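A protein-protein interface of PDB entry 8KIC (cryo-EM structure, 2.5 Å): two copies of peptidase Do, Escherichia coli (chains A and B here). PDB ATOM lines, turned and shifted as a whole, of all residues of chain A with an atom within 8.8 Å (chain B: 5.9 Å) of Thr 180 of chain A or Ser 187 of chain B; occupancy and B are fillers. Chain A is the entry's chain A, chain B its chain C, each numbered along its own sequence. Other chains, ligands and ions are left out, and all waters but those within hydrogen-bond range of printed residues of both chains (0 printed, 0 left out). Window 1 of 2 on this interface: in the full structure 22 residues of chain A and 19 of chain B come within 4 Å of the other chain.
Thr 180 of chain A touches just these residues of chain B: Ser 187 (3.7 Å), Arg 191 (3.2 Å) and Gln 204 (3.7 Å).
No residue of chain A comes within 4 Å of Val 186 of chain B.
Of the printed residues of chain A, Val 164 of chain B touches Leu 46.
Printed residues of chain A within 4 Å of Arg 191 of chain B: Leu 177 (3.8 Å), Gly 178 (3.4 Å), Gln 179 (3.1 Å) and Thr 180 (3.2 Å).
Printed residues of chain A within 4 Å of Ile 185 of chain B: Ala 181.
Of the printed residues of chain A, Gly 165 of chain B touches Leu 46.
The nearest printed residue of chain A that does not touch Ile 242 of chain B is Pro 174 of chain A (4.5 Å).
The side-chain hydroxyl (OG) of Ser 187 of chain B sits at hydrogen-bond distance from the backbone carbonyl oxygen (O) of Ala 181 of chain A.
O of Gly 178 of chain A lies close to NH2 of Arg 191 of chain B, at 3.4 Å.
O of Gln 179 of chain A sits at hydrogen-bond distance from NH2 of Arg 191 of chain B (3.1 Å).
NH2 of Arg 191 of chain B is in hydrogen-bond range of OG1 of Thr 180 of chain A (3.2 Å).
No position is printed for both chains.
Of the 11 pairs that touch across the chains among the printed residues, none has its exchanged pair printed and touching as well.
Of the 29 printed residues of chain A, 6 touch a printed residue of chain B.
Printed residues of chain A that touch a printed residue of chain B: Leu 46, Leu 177, Gly 178, Gln 179, Thr 180 and Ala 181.
Hydrophobic or aromatic side chains of chain A that line the printed part of chain B: Leu 46 and Leu 177.
N of Asp 206 of chain B sits at hydrogen-bond distance from O of Ile 185 of chain B (3.5 Å).
The backbone carbonyl oxygen (O) of Ala 188 of chain B is in hydrogen-bond range of the backbone NH (N) of Gln 204 of chain B, 3.2 Å away.
NE of Arg 191 of chain B is in hydrogen-bond range of OE1 of Gln 204 of chain B (2.8 Å).
NE2 of Gln 179 of chain A sits at hydrogen-bond distance from O of Leu 50 of chain A, at 2.9 Å.
The side-chain amide nitrogen (NE2) of Gln 179 of chain A sits at hydrogen-bond distance from the backbone carbonyl oxygen (O) of Val 53 of chain A, at 3.1 Å.
The backbone NH (N) of Thr 180 of chain A sits at hydrogen-bond distance from the backbone carbonyl oxygen (O) of Gly 172 of chain A (2.9 Å).
O of Val 164 of chain B touches CD1 of Leu 46 of chain A, 3.9 Å away.
Leu 46 of chain A touches Gly 165 of chain B.
CZ of Arg 191 of chain B touches O of Leu 177 of chain A (3.8 Å).
CD1 of Leu 177 of chain A touches CG2 of Ile 242 of chain B (3.9 Å).
Ser 187 of chain B touches Thr 180 of chain A.
OG1 of Thr 180 of chain A touches NE2 of Gln 204 of chain B, at 3.7 Å.
Ala 181 of chain A touches Ile 185 of chain B (O to CD1, 3.4 Å).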
ATOM      1  N   LEU A  46       2.143   0.009 -10.219  1.00  0.00           N
ATOM      2  CA  LEU A  46       0.839  -0.571 -10.510  1.00  0.00           C
ATOM      3  C   LEU A  46       0.485  -0.466 -11.985  1.00  0.00           C
ATOM      4  O   LEU A  46      -0.300  -1.274 -12.487  1.00  0.00           O
ATOM      5  CB  LEU A  46      -0.239   0.107  -9.664  1.00  0.00           C
ATOM      6  CG  LEU A  46      -0.404  -0.381  -8.225  1.00  0.00           C
ATOM      7  CD1 LEU A  46      -1.332   0.531  -7.455  1.00  0.00           C
ATOM      8  CD2 LEU A  46      -0.913  -1.809  -8.191  1.00  0.00           C
ATOM      9  N   LEU A  50      -1.202  -4.187 -13.376  1.00  0.00           N
ATOM     10  CA  LEU A  50      -2.663  -4.238 -13.353  1.00  0.00           C
ATOM     11  C   LEU A  50      -3.291  -4.984 -14.527  1.00  0.00           C
ATOM     12  O   LEU A  50      -4.304  -5.668 -14.304  1.00  0.00           O
ATOM     13  CB  LEU A  50      -3.233  -2.815 -13.262  1.00  0.00           C
ATOM     14  CG  LEU A  50      -3.244  -2.146 -11.887  1.00  0.00           C
ATOM     15  CD1 LEU A  50      -3.778  -0.733 -11.992  1.00  0.00           C
ATOM     16  CD2 LEU A  50      -4.043  -2.943 -10.881  1.00  0.00           C
ATOM     17  N   VAL A  53      -4.289  -8.891 -13.935  1.00  0.00           N
ATOM     18  CA  VAL A  53      -5.332  -9.350 -13.025  1.00  0.00           C
ATOM     19  C   VAL A  53      -6.676  -9.161 -13.708  1.00  0.00           C
ATOM     20  O   VAL A  53      -6.973  -8.072 -14.213  1.00  0.00           O
ATOM     21  CB  VAL A  53      -5.285  -8.601 -11.682  1.00  0.00           C
ATOM     22  CG1 VAL A  53      -6.304  -9.171 -10.718  1.00  0.00           C
ATOM     23  CG2 VAL A  53      -3.899  -8.678 -11.090  1.00  0.00           C
ATOM     24  N   SER A  93     -12.042 -13.242  -9.170  1.00  0.00           N
ATOM     25  CA  SER A  93     -10.865 -12.682  -9.816  1.00  0.00           C
ATOM     26  C   SER A  93      -9.942 -13.800 -10.296  1.00  0.00           C
ATOM     27  O   SER A  93     -10.211 -14.983 -10.109  1.00  0.00           O
ATOM     28  CB  SER A  93     -10.138 -11.732  -8.865  1.00  0.00           C
ATOM     29  OG  SER A  93     -11.018 -10.756  -8.349  1.00  0.00           O
ATOM     30  N   ASN A 122      -9.197  -5.531 -17.941  1.00  0.00           N
ATOM     31  CA  ASN A 122      -9.467  -4.210 -17.387  1.00  0.00           C
ATOM     32  C   ASN A 122      -9.603  -3.134 -18.458  1.00  0.00           C
ATOM     33  O   ASN A 122     -10.013  -2.013 -18.139  1.00  0.00           O
ATOM     34  CB  ASN A 122      -8.388  -3.819 -16.367  1.00  0.00           C
ATOM     35  CG  ASN A 122      -7.048  -3.507 -17.003  1.00  0.00           C
ATOM     36  OD1 ASN A 122      -6.827  -3.741 -18.190  1.00  0.00           O
ATOM     37  ND2 ASN A 122      -6.139  -2.964 -16.202  1.00  0.00           N
ATOM     38  N   VAL A 169      -0.087  -5.181  -1.457  1.00  0.00           N
ATOM     39  CA  VAL A 169      -1.175  -4.579  -2.222  1.00  0.00           C
ATOM     40  C   VAL A 169      -2.101  -5.688  -2.696  1.00  0.00           C
ATOM     41  O   VAL A 169      -1.647  -6.669  -3.290  1.00  0.00           O
ATOM     42  CB  VAL A 169      -0.651  -3.759  -3.418  1.00  0.00           C
ATOM     43  CG1 VAL A 169      -1.789  -3.039  -4.115  1.00  0.00           C
ATOM     44  CG2 VAL A 169       0.394  -2.767  -2.965  1.00  0.00           C
ATOM     45  N   ALA A 170      -3.392  -5.532  -2.440  1.00  0.00           N
ATOM     46  CA  ALA A 170      -4.403  -6.481  -2.883  1.00  0.00           C
ATOM     47  C   ALA A 170      -5.137  -5.906  -4.088  1.00  0.00           C
ATOM     48  O   ALA A 170      -5.635  -4.779  -4.035  1.00  0.00           O
ATOM     49  CB  ALA A 170      -5.385  -6.794  -1.757  1.00  0.00           C
ATOM     50  N   VAL A 171      -5.201  -6.675  -5.171  1.00  0.00           N
ATOM     51  CA  VAL A 171      -5.910  -6.277  -6.380  1.00  0.00           C
ATOM     52  C   VAL A 171      -7.012  -7.289  -6.651  1.00  0.00           C
ATOM     53  O   VAL A 171      -6.753  -8.499  -6.719  1.00  0.00           O
ATOM     54  CB  VAL A 171      -4.965  -6.156  -7.586  1.00  0.00           C
ATOM     55  CG1 VAL A 171      -5.687  -5.501  -8.744  1.00  0.00           C
ATOM     56  CG2 VAL A 171      -3.734  -5.361  -7.213  1.00  0.00           C
ATOM     57  N   GLY A 172      -8.229  -6.792  -6.811  1.00  0.00           N
ATOM     58  CA  GLY A 172      -9.377  -7.650  -6.987  1.00  0.00           C
ATOM     59  C   GLY A 172     -10.568  -6.918  -7.554  1.00  0.00           C
ATOM     60  O   GLY A 172     -10.429  -5.918  -8.257  1.00  0.00           O
ATOM     61  N   ASN A 173     -11.756  -7.419  -7.218  1.00  0.00           N
ATOM     62  CA  ASN A 173     -13.009  -6.991  -7.847  1.00  0.00           C
ATOM     63  C   ASN A 173     -14.157  -7.044  -6.851  1.00  0.00           C
ATOM     64  O   ASN A 173     -15.132  -7.776  -7.045  1.00  0.00           O
ATOM     65  CB  ASN A 173     -13.318  -7.868  -9.061  1.00  0.00           C
ATOM     66  CG  ASN A 173     -13.899  -7.093 -10.213  1.00  0.00           C
ATOM     67  OD1 ASN A 173     -13.295  -6.991 -11.277  1.00  0.00           O
ATOM     68  ND2 ASN A 173     -15.088  -6.543 -10.010  1.00  0.00           N
ATOM     69  N   PRO A 174     -14.099  -6.245  -5.786  1.00  0.00           N
ATOM     70  CA  PRO A 174     -15.118  -6.348  -4.733  1.00  0.00           C
ATOM     71  C   PRO A 174     -16.483  -5.809  -5.137  1.00  0.00           C
ATOM     72  O   PRO A 174     -16.613  -4.734  -5.726  1.00  0.00           O
ATOM     73  CB  PRO A 174     -14.518  -5.509  -3.597  1.00  0.00           C
ATOM     74  CG  PRO A 174     -13.675  -4.513  -4.273  1.00  0.00           C
ATOM     75  CD  PRO A 174     -13.182  -5.115  -5.556  1.00  0.00           C
ATOM     76  N   PHE A 175     -17.515  -6.587  -4.807  1.00  0.00           N
ATOM     77  CA  PHE A 175     -18.924  -6.234  -4.999  1.00  0.00           C
ATOM     78  C   PHE A 175     -19.281  -5.985  -6.463  1.00  0.00           C
ATOM     79  O   PHE A 175     -20.331  -5.411  -6.756  1.00  0.00           O
ATOM     80  CB  PHE A 175     -19.321  -5.019  -4.146  1.00  0.00           C
ATOM     81  CG  PHE A 175     -19.136  -5.227  -2.671  1.00  0.00           C
ATOM     82  CD1 PHE A 175     -19.881  -6.167  -1.991  1.00  0.00           C
ATOM     83  CD2 PHE A 175     -18.208  -4.485  -1.967  1.00  0.00           C
ATOM     84  CE1 PHE A 175     -19.702  -6.364  -0.640  1.00  0.00           C
ATOM     85  CE2 PHE A 175     -18.029  -4.680  -0.617  1.00  0.00           C
ATOM     86  CZ  PHE A 175     -18.777  -5.619   0.045  1.00  0.00           C
ATOM     87  N   GLY A 176     -18.435  -6.411  -7.395  1.00  0.00           N
ATOM     88  CA  GLY A 176     -18.719  -6.225  -8.802  1.00  0.00           C
ATOM     89  C   GLY A 176     -18.537  -4.822  -9.327  1.00  0.00           C
ATOM     90  O   GLY A 176     -19.102  -4.489 -10.371  1.00  0.00           O
ATOM     91  N   LEU A 177     -17.763  -3.981  -8.638  1.00  0.00           N
ATOM     92  CA  LEU A 177     -17.560  -2.611  -9.097  1.00  0.00           C
ATOM     93  C   LEU A 177     -16.582  -2.540 -10.262  1.00  0.00           C
ATOM     94  O   LEU A 177     -16.760  -1.730 -11.177  1.00  0.00           O
ATOM     95  CB  LEU A 177     -17.067  -1.737  -7.942  1.00  0.00           C
ATOM     96  CG  LEU A 177     -18.046  -1.484  -6.796  1.00  0.00           C
ATOM     97  CD1 LEU A 177     -17.323  -0.979  -5.567  1.00  0.00           C
ATOM     98  CD2 LEU A 177     -19.110  -0.496  -7.224  1.00  0.00           C
ATOM     99  N   GLY A 178     -15.554  -3.373 -10.251  1.00  0.00           N
ATOM    100  CA  GLY A 178     -14.467  -3.323 -11.196  1.00  0.00           C
ATOM    101  C   GLY A 178     -13.153  -3.486 -10.478  1.00  0.00           C
ATOM    102  O   GLY A 178     -13.103  -3.713  -9.266  1.00  0.00           O
ATOM    103  N   GLN A 179     -12.064  -3.352 -11.227  1.00  0.00           N
ATOM    104  CA  GLN A 179     -10.739  -3.593 -10.671  1.00  0.00           C
ATOM    105  C   GLN A 179     -10.393  -2.556  -9.606  1.00  0.00           C
ATOM    106  O   GLN A 179     -10.457  -1.349  -9.850  1.00  0.00           O
ATOM    107  CB  GLN A 179      -9.695  -3.583 -11.782  1.00  0.00           C
ATOM    108  CG  GLN A 179      -8.350  -4.122 -11.361  1.00  0.00           C
ATOM    109  CD  GLN A 179      -7.336  -4.090 -12.478  1.00  0.00           C
ATOM    110  OE1 GLN A 179      -6.999  -3.028 -12.991  1.00  0.00           O
ATOM    111  NE2 GLN A 179      -6.831  -5.257 -12.852  1.00  0.00           N
ATOM    112  N   THR A 180     -10.012  -3.037  -8.424  1.00  0.00           N
ATOM    113  CA  THR A 180      -9.738  -2.193  -7.271  1.00  0.00           C
ATOM    114  C   THR A 180      -8.430  -2.631  -6.627  1.00  0.00           C
ATOM    115  O   THR A 180      -8.102  -3.822  -6.624  1.00  0.00           O
ATOM    116  CB  THR A 180     -10.891  -2.272  -6.254  1.00  0.00           C
ATOM    117  OG1 THR A 180     -12.098  -1.800  -6.859  1.00  0.00           O
ATOM    118  CG2 THR A 180     -10.611  -1.438  -5.028  1.00  0.00           C
ATOM    119  N   ALA A 181      -7.690  -1.664  -6.084  1.00  0.00           N
ATOM    120  CA  ALA A 181      -6.437  -1.899  -5.375  1.00  0.00           C
ATOM    121  C   ALA A 181      -6.502  -1.315  -3.967  1.00  0.00           C
ATOM    122  O   ALA A 181      -6.889  -0.158  -3.790  1.00  0.00           O
ATOM    123  CB  ALA A 181      -5.261  -1.292  -6.138  1.00  0.00           C
ATOM    124  N   THR A 182      -6.109  -2.113  -2.974  1.00  0.00           N
ATOM    125  CA  THR A 182      -6.014  -1.686  -1.581  1.00  0.00           C
ATOM    126  C   THR A 182      -4.634  -2.041  -1.039  1.00  0.00           C
ATOM    127  O   THR A 182      -3.899  -2.822  -1.640  1.00  0.00           O
ATOM    128  CB  THR A 182      -7.107  -2.321  -0.702  1.00  0.00           C
ATOM    129  OG1 THR A 182      -7.051  -3.746  -0.800  1.00  0.00           O
ATOM    130  CG2 THR A 182      -8.485  -1.850  -1.126  1.00  0.00           C
ATOM    131  N   SER A 183      -4.278  -1.462   0.108  1.00  0.00           N
ATOM    132  CA  SER A 183      -2.921  -1.564   0.636  1.00  0.00           C
ATOM    133  C   SER A 183      -2.923  -1.935   2.116  1.00  0.00           C
ATOM    134  O   SER A 183      -3.860  -1.617   2.850  1.00  0.00           O
ATOM    135  CB  SER A 183      -2.162  -0.254   0.434  1.00  0.00           C
ATOM    136  OG  SER A 183      -0.776  -0.433   0.642  1.00  0.00           O
ATOM    137  N   SER A 208      -7.862  -4.294   2.742  1.00  0.00           N
ATOM    138  CA  SER A 208      -9.311  -4.463   2.658  1.00  0.00           C
ATOM    139  C   SER A 208      -9.640  -5.500   1.592  1.00  0.00           C
ATOM    140  O   SER A 208      -9.382  -5.283   0.405  1.00  0.00           O
ATOM    141  CB  SER A 208      -9.990  -3.134   2.345  1.00  0.00           C
ATOM    142  OG  SER A 208      -9.816  -2.205   3.393  1.00  0.00           O
ATOM    143  N   ILE A 209     -10.205  -6.626   2.011  1.00  0.00           N
ATOM    144  CA  ILE A 209     -10.614  -7.696   1.110  1.00  0.00           C
ATOM    145  C   ILE A 209     -12.070  -8.018   1.411  1.00  0.00           C
ATOM    146  O   ILE A 209     -12.426  -8.289   2.563  1.00  0.00           O
ATOM    147  CB  ILE A 209      -9.719  -8.936   1.251  1.00  0.00           C
ATOM    148  CG1 ILE A 209      -8.395  -8.714   0.523  1.00  0.00           C
ATOM    149  CG2 ILE A 209     -10.402 -10.160   0.689  1.00  0.00           C
ATOM    150  CD1 ILE A 209      -7.195  -9.185   1.288  1.00  0.00           C
ATOM    151  N   ASN A 210     -12.904  -7.984   0.381  1.00  0.00           N
ATOM    152  CA  ASN A 210     -14.347  -8.111   0.508  1.00  0.00           C
ATOM    153  C   ASN A 210     -14.851  -9.221  -0.415  1.00  0.00           C
ATOM    154  O   ASN A 210     -14.075  -9.995  -0.974  1.00  0.00           O
ATOM    155  CB  ASN A 210     -15.018  -6.771   0.205  1.00  0.00           C
ATOM    156  CG  ASN A 210     -14.876  -5.779   1.340  1.00  0.00           C
ATOM    157  OD1 ASN A 210     -15.518  -5.914   2.375  1.00  0.00           O
ATOM    158  ND2 ASN A 210     -14.037  -4.772   1.146  1.00  0.00           N
ATOM    159  N   GLY A 212     -16.019 -10.885  -3.677  1.00  0.00           N
ATOM    160  CA  GLY A 212     -15.587 -10.671  -5.035  1.00  0.00           C
ATOM    161  C   GLY A 212     -14.085 -10.618  -5.213  1.00  0.00           C
ATOM    162  O   GLY A 212     -13.610 -10.609  -6.349  1.00  0.00           O
ATOM    163  N   ASN A 213     -13.331 -10.594  -4.115  1.00  0.00           N
ATOM    164  CA  ASN A 213     -11.876 -10.517  -4.145  1.00  0.00           C
ATOM    165  C   ASN A 213     -11.194 -11.875  -4.252  1.00  0.00           C
ATOM    166  O   ASN A 213      -9.980 -11.914  -4.477  1.00  0.00           O
ATOM    167  CB  ASN A 213     -11.370  -9.808  -2.887  1.00  0.00           C
ATOM    168  CG  ASN A 213     -11.119  -8.335  -3.103  1.00  0.00           C
ATOM    169  OD1 ASN A 213     -10.320  -7.951  -3.944  1.00  0.00           O
ATOM    170  ND2 ASN A 213     -11.787  -7.502  -2.326  1.00  0.00           N
ATOM    171  N   GLY A 216      -7.937 -13.225  -6.594  1.00  0.00           N
ATOM    172  CA  GLY A 216      -7.139 -12.092  -7.017  1.00  0.00           C
ATOM    173  C   GLY A 216      -5.738 -12.069  -6.449  1.00  0.00           C
ATOM    174  O   GLY A 216      -5.301 -13.035  -5.823  1.00  0.00           O
ATOM    175  N   ALA A 217      -5.029 -10.957  -6.639  1.00  0.00           N
ATOM    176  CA  ALA A 217      -3.589 -10.919  -6.432  1.00  0.00           C
ATOM    177  C   ALA A 217      -3.228 -10.225  -5.129  1.00  0.00           C
ATOM    178  O   ALA A 217      -3.839  -9.221  -4.757  1.00  0.00           O
ATOM    179  CB  ALA A 217      -2.889 -10.211  -7.590  1.00  0.00           C
ATOM    180  N   LEU A 219       0.361  -8.647  -3.836  1.00  0.00           N
ATOM    181  CA  LEU A 219       1.638  -8.281  -4.423  1.00  0.00           C
ATOM    182  C   LEU A 219       2.508  -7.566  -3.402  1.00  0.00           C
ATOM    183  O   LEU A 219       2.011  -6.949  -2.458  1.00  0.00           O
ATOM    184  CB  LEU A 219       1.448  -7.370  -5.645  1.00  0.00           C
ATOM    185  CG  LEU A 219       0.388  -7.718  -6.689  1.00  0.00           C
ATOM    186  CD1 LEU A 219       0.016  -6.476  -7.467  1.00  0.00           C
ATOM    187  CD2 LEU A 219       0.867  -8.809  -7.626  1.00  0.00           C
ATOM    188  N   ASN A 229      -5.588 -14.451  -2.854  1.00  0.00           N
ATOM    189  CA  ASN A 229      -6.575 -14.152  -1.820  1.00  0.00           C
ATOM    190  C   ASN A 229      -7.657 -15.224  -1.772  1.00  0.00           C
ATOM    191  O   ASN A 229      -8.240 -15.577  -2.799  1.00  0.00           O
ATOM    192  CB  ASN A 229      -7.203 -12.782  -2.067  1.00  0.00           C
ATOM    193  CG  ASN A 229      -6.193 -11.657  -2.005  1.00  0.00           C
ATOM    194  OD1 ASN A 229      -5.314 -11.646  -1.152  1.00  0.00           O
ATOM    195  ND2 ASN A 229      -6.326 -10.694  -2.903  1.00  0.00           N
ATOM    196  N   VAL B 164      -4.191   5.764 -10.155  1.00  0.00           N
ATOM    197  CA  VAL B 164      -4.476   4.733  -9.165  1.00  0.00           C
ATOM    198  C   VAL B 164      -3.183   4.331  -8.472  1.00  0.00           C
ATOM    199  O   VAL B 164      -2.222   3.894  -9.116  1.00  0.00           O
ATOM    200  CB  VAL B 164      -5.163   3.527  -9.823  1.00  0.00           C
ATOM    201  CG1 VAL B 164      -5.206   2.348  -8.865  1.00  0.00           C
ATOM    202  CG2 VAL B 164      -6.555   3.902 -10.263  1.00  0.00           C
ATOM    203  N   GLY B 165      -3.158   4.466  -7.148  1.00  0.00           N
ATOM    204  CA  GLY B 165      -1.974   4.218  -6.354  1.00  0.00           C
ATOM    205  C   GLY B 165      -1.449   5.428  -5.618  1.00  0.00           C
ATOM    206  O   GLY B 165      -0.535   5.280  -4.800  1.00  0.00           O
ATOM    207  N   ILE B 185      -5.232   4.995  -0.037  1.00  0.00           N
ATOM    208  CA  ILE B 185      -4.797   5.210  -1.412  1.00  0.00           C
ATOM    209  C   ILE B 185      -6.020   5.417  -2.299  1.00  0.00           C
ATOM    210  O   ILE B 185      -7.150   5.113  -1.923  1.00  0.00           O
ATOM    211  CB  ILE B 185      -3.927   4.054  -1.958  1.00  0.00           C
ATOM    212  CG1 ILE B 185      -4.725   2.752  -2.034  1.00  0.00           C
ATOM    213  CG2 ILE B 185      -2.671   3.874  -1.135  1.00  0.00           C
ATOM    214  CD1 ILE B 185      -4.175   1.767  -3.027  1.00  0.00           C
ATOM    215  N   VAL B 186      -5.772   5.956  -3.487  1.00  0.00           N
ATOM    216  CA  VAL B 186      -6.784   6.018  -4.537  1.00  0.00           C
ATOM    217  C   VAL B 186      -6.904   4.630  -5.155  1.00  0.00           C
ATOM    218  O   VAL B 186      -5.934   4.096  -5.700  1.00  0.00           O
ATOM    219  CB  VAL B 186      -6.419   7.069  -5.597  1.00  0.00           C
ATOM    220  CG1 VAL B 186      -7.383   7.011  -6.766  1.00  0.00           C
ATOM    221  CG2 VAL B 186      -6.398   8.454  -4.986  1.00  0.00           C
ATOM    222  N   SER B 187      -8.094   4.040  -5.064  1.00  0.00           N
ATOM    223  CA  SER B 187      -8.333   2.674  -5.503  1.00  0.00           C
ATOM    224  C   SER B 187      -8.785   2.598  -6.953  1.00  0.00           C
ATOM    225  O   SER B 187      -8.430   1.651  -7.661  1.00  0.00           O
ATOM    226  CB  SER B 187      -9.383   2.018  -4.606  1.00  0.00           C
ATOM    227  OG  SER B 187      -8.867   1.777  -3.315  1.00  0.00           O
ATOM    228  N   ALA B 188      -9.562   3.579  -7.404  1.00  0.00           N
ATOM    229  CA  ALA B 188     -10.141   3.570  -8.737  1.00  0.00           C
ATOM    230  C   ALA B 188     -10.499   4.995  -9.126  1.00  0.00           C
ATOM    231  O   ALA B 188     -10.542   5.894  -8.285  1.00  0.00           O
ATOM    232  CB  ALA B 188     -11.371   2.663  -8.805  1.00  0.00           C
ATOM    233  N   LEU B 189     -10.746   5.190 -10.417  1.00  0.00           N
ATOM    234  CA  LEU B 189     -11.127   6.481 -10.962  1.00  0.00           C
ATOM    235  C   LEU B 189     -12.310   6.310 -11.901  1.00  0.00           C
ATOM    236  O   LEU B 189     -12.515   5.247 -12.487  1.00  0.00           O
ATOM    237  CB  LEU B 189      -9.964   7.145 -11.709  1.00  0.00           C
ATOM    238  CG  LEU B 189      -8.695   7.455 -10.923  1.00  0.00           C
ATOM    239  CD1 LEU B 189      -7.520   7.617 -11.854  1.00  0.00           C
ATOM    240  CD2 LEU B 189      -8.887   8.702 -10.084  1.00  0.00           C
ATOM    241  N   ARG B 191     -15.524   6.211 -11.268  1.00  0.00           N
ATOM    242  CA  ARG B 191     -16.565   5.302 -10.812  1.00  0.00           C
ATOM    243  C   ARG B 191     -17.935   5.954 -10.923  1.00  0.00           C
ATOM    244  O   ARG B 191     -18.092   7.150 -10.665  1.00  0.00           O
ATOM    245  CB  ARG B 191     -16.294   4.876  -9.371  1.00  0.00           C
ATOM    246  CG  ARG B 191     -15.241   3.796  -9.243  1.00  0.00           C
ATOM    247  CD  ARG B 191     -15.747   2.470  -9.784  1.00  0.00           C
ATOM    248  NE  ARG B 191     -14.960   1.350  -9.284  1.00  0.00           N
ATOM    249  CZ  ARG B 191     -14.049   0.693  -9.986  1.00  0.00           C
ATOM    250  NH1 ARG B 191     -13.802   0.988 -11.250  1.00  0.00           N
ATOM    251  NH2 ARG B 191     -13.372  -0.287  -9.404  1.00  0.00           N
ATOM    252  N   GLN B 204     -12.674   6.692  -6.048  1.00  0.00           N
ATOM    253  CA  GLN B 204     -12.828   5.646  -5.048  1.00  0.00           C
ATOM    254  C   GLN B 204     -11.577   5.574  -4.182  1.00  0.00           C
ATOM    255  O   GLN B 204     -10.457   5.654  -4.690  1.00  0.00           O
ATOM    256  CB  GLN B 204     -13.103   4.299  -5.711  1.00  0.00           C
ATOM    257  CG  GLN B 204     -13.744   3.286  -4.794  1.00  0.00           C
ATOM    258  CD  GLN B 204     -14.005   1.967  -5.481  1.00  0.00           C
ATOM    259  OE1 GLN B 204     -14.595   1.923  -6.554  1.00  0.00           O
ATOM    260  NE2 GLN B 204     -13.570   0.883  -4.863  1.00  0.00           N
ATOM    261  N   THR B 205     -11.772   5.428  -2.876  1.00  0.00           N
ATOM    262  CA  THR B 205     -10.670   5.401  -1.926  1.00  0.00           C
ATOM    263  C   THR B 205     -10.973   4.398  -0.824  1.00  0.00           C
ATOM    264  O   THR B 205     -12.133   4.064  -0.573  1.00  0.00           O
ATOM    265  CB  THR B 205     -10.414   6.799  -1.325  1.00  0.00           C
ATOM    266  OG1 THR B 205      -9.324   6.740  -0.401  1.00  0.00           O
ATOM    267  CG2 THR B 205     -11.647   7.312  -0.602  1.00  0.00           C
ATOM    268  N   ASP B 206      -9.917   3.909  -0.174  1.00  0.00           N
ATOM    269  CA  ASP B 206     -10.054   3.002   0.959  1.00  0.00           C
ATOM    270  C   ASP B 206      -9.641   3.630   2.284  1.00  0.00           C
ATOM    271  O   ASP B 206      -9.429   2.906   3.260  1.00  0.00           O
ATOM    272  CB  ASP B 206      -9.265   1.711   0.723  1.00  0.00           C
ATOM    273  CG  ASP B 206      -7.869   1.959   0.221  1.00  0.00           C
ATOM    274  OD1 ASP B 206      -7.735   2.615  -0.827  1.00  0.00           O
ATOM    275  OD2 ASP B 206      -6.907   1.496   0.866  1.00  0.00           O
ATOM    276  N   GLY B 241     -14.067  -0.039   3.634  1.00  0.00           N
ATOM    277  CA  GLY B 241     -12.984   0.365   2.771  1.00  0.00           C
ATOM    278  C   GLY B 241     -13.362   0.761   1.364  1.00  0.00           C
ATOM    279  O   GLY B 241     -12.501   0.701   0.484  1.00  0.00           O
ATOM    280  N   ILE B 242     -14.608   1.167   1.122  1.00  0.00           N
ATOM    281  CA  ILE B 242     -15.078   1.579  -0.202  1.00  0.00           C
ATOM    282  C   ILE B 242     -15.761   2.934  -0.023  1.00  0.00           C
ATOM    283  O   ILE B 242     -16.923   2.994   0.389  1.00  0.00           O
ATOM    284  CB  ILE B 242     -16.049   0.566  -0.825  1.00  0.00           C
ATOM    285  CG1 ILE B 242     -15.523  -0.876  -0.775  1.00  0.00           C
ATOM    286  CG2 ILE B 242     -16.340   0.939  -2.264  1.00  0.00           C
ATOM    287  CD1 ILE B 242     -14.191  -1.104  -1.419  1.00  0.00           C
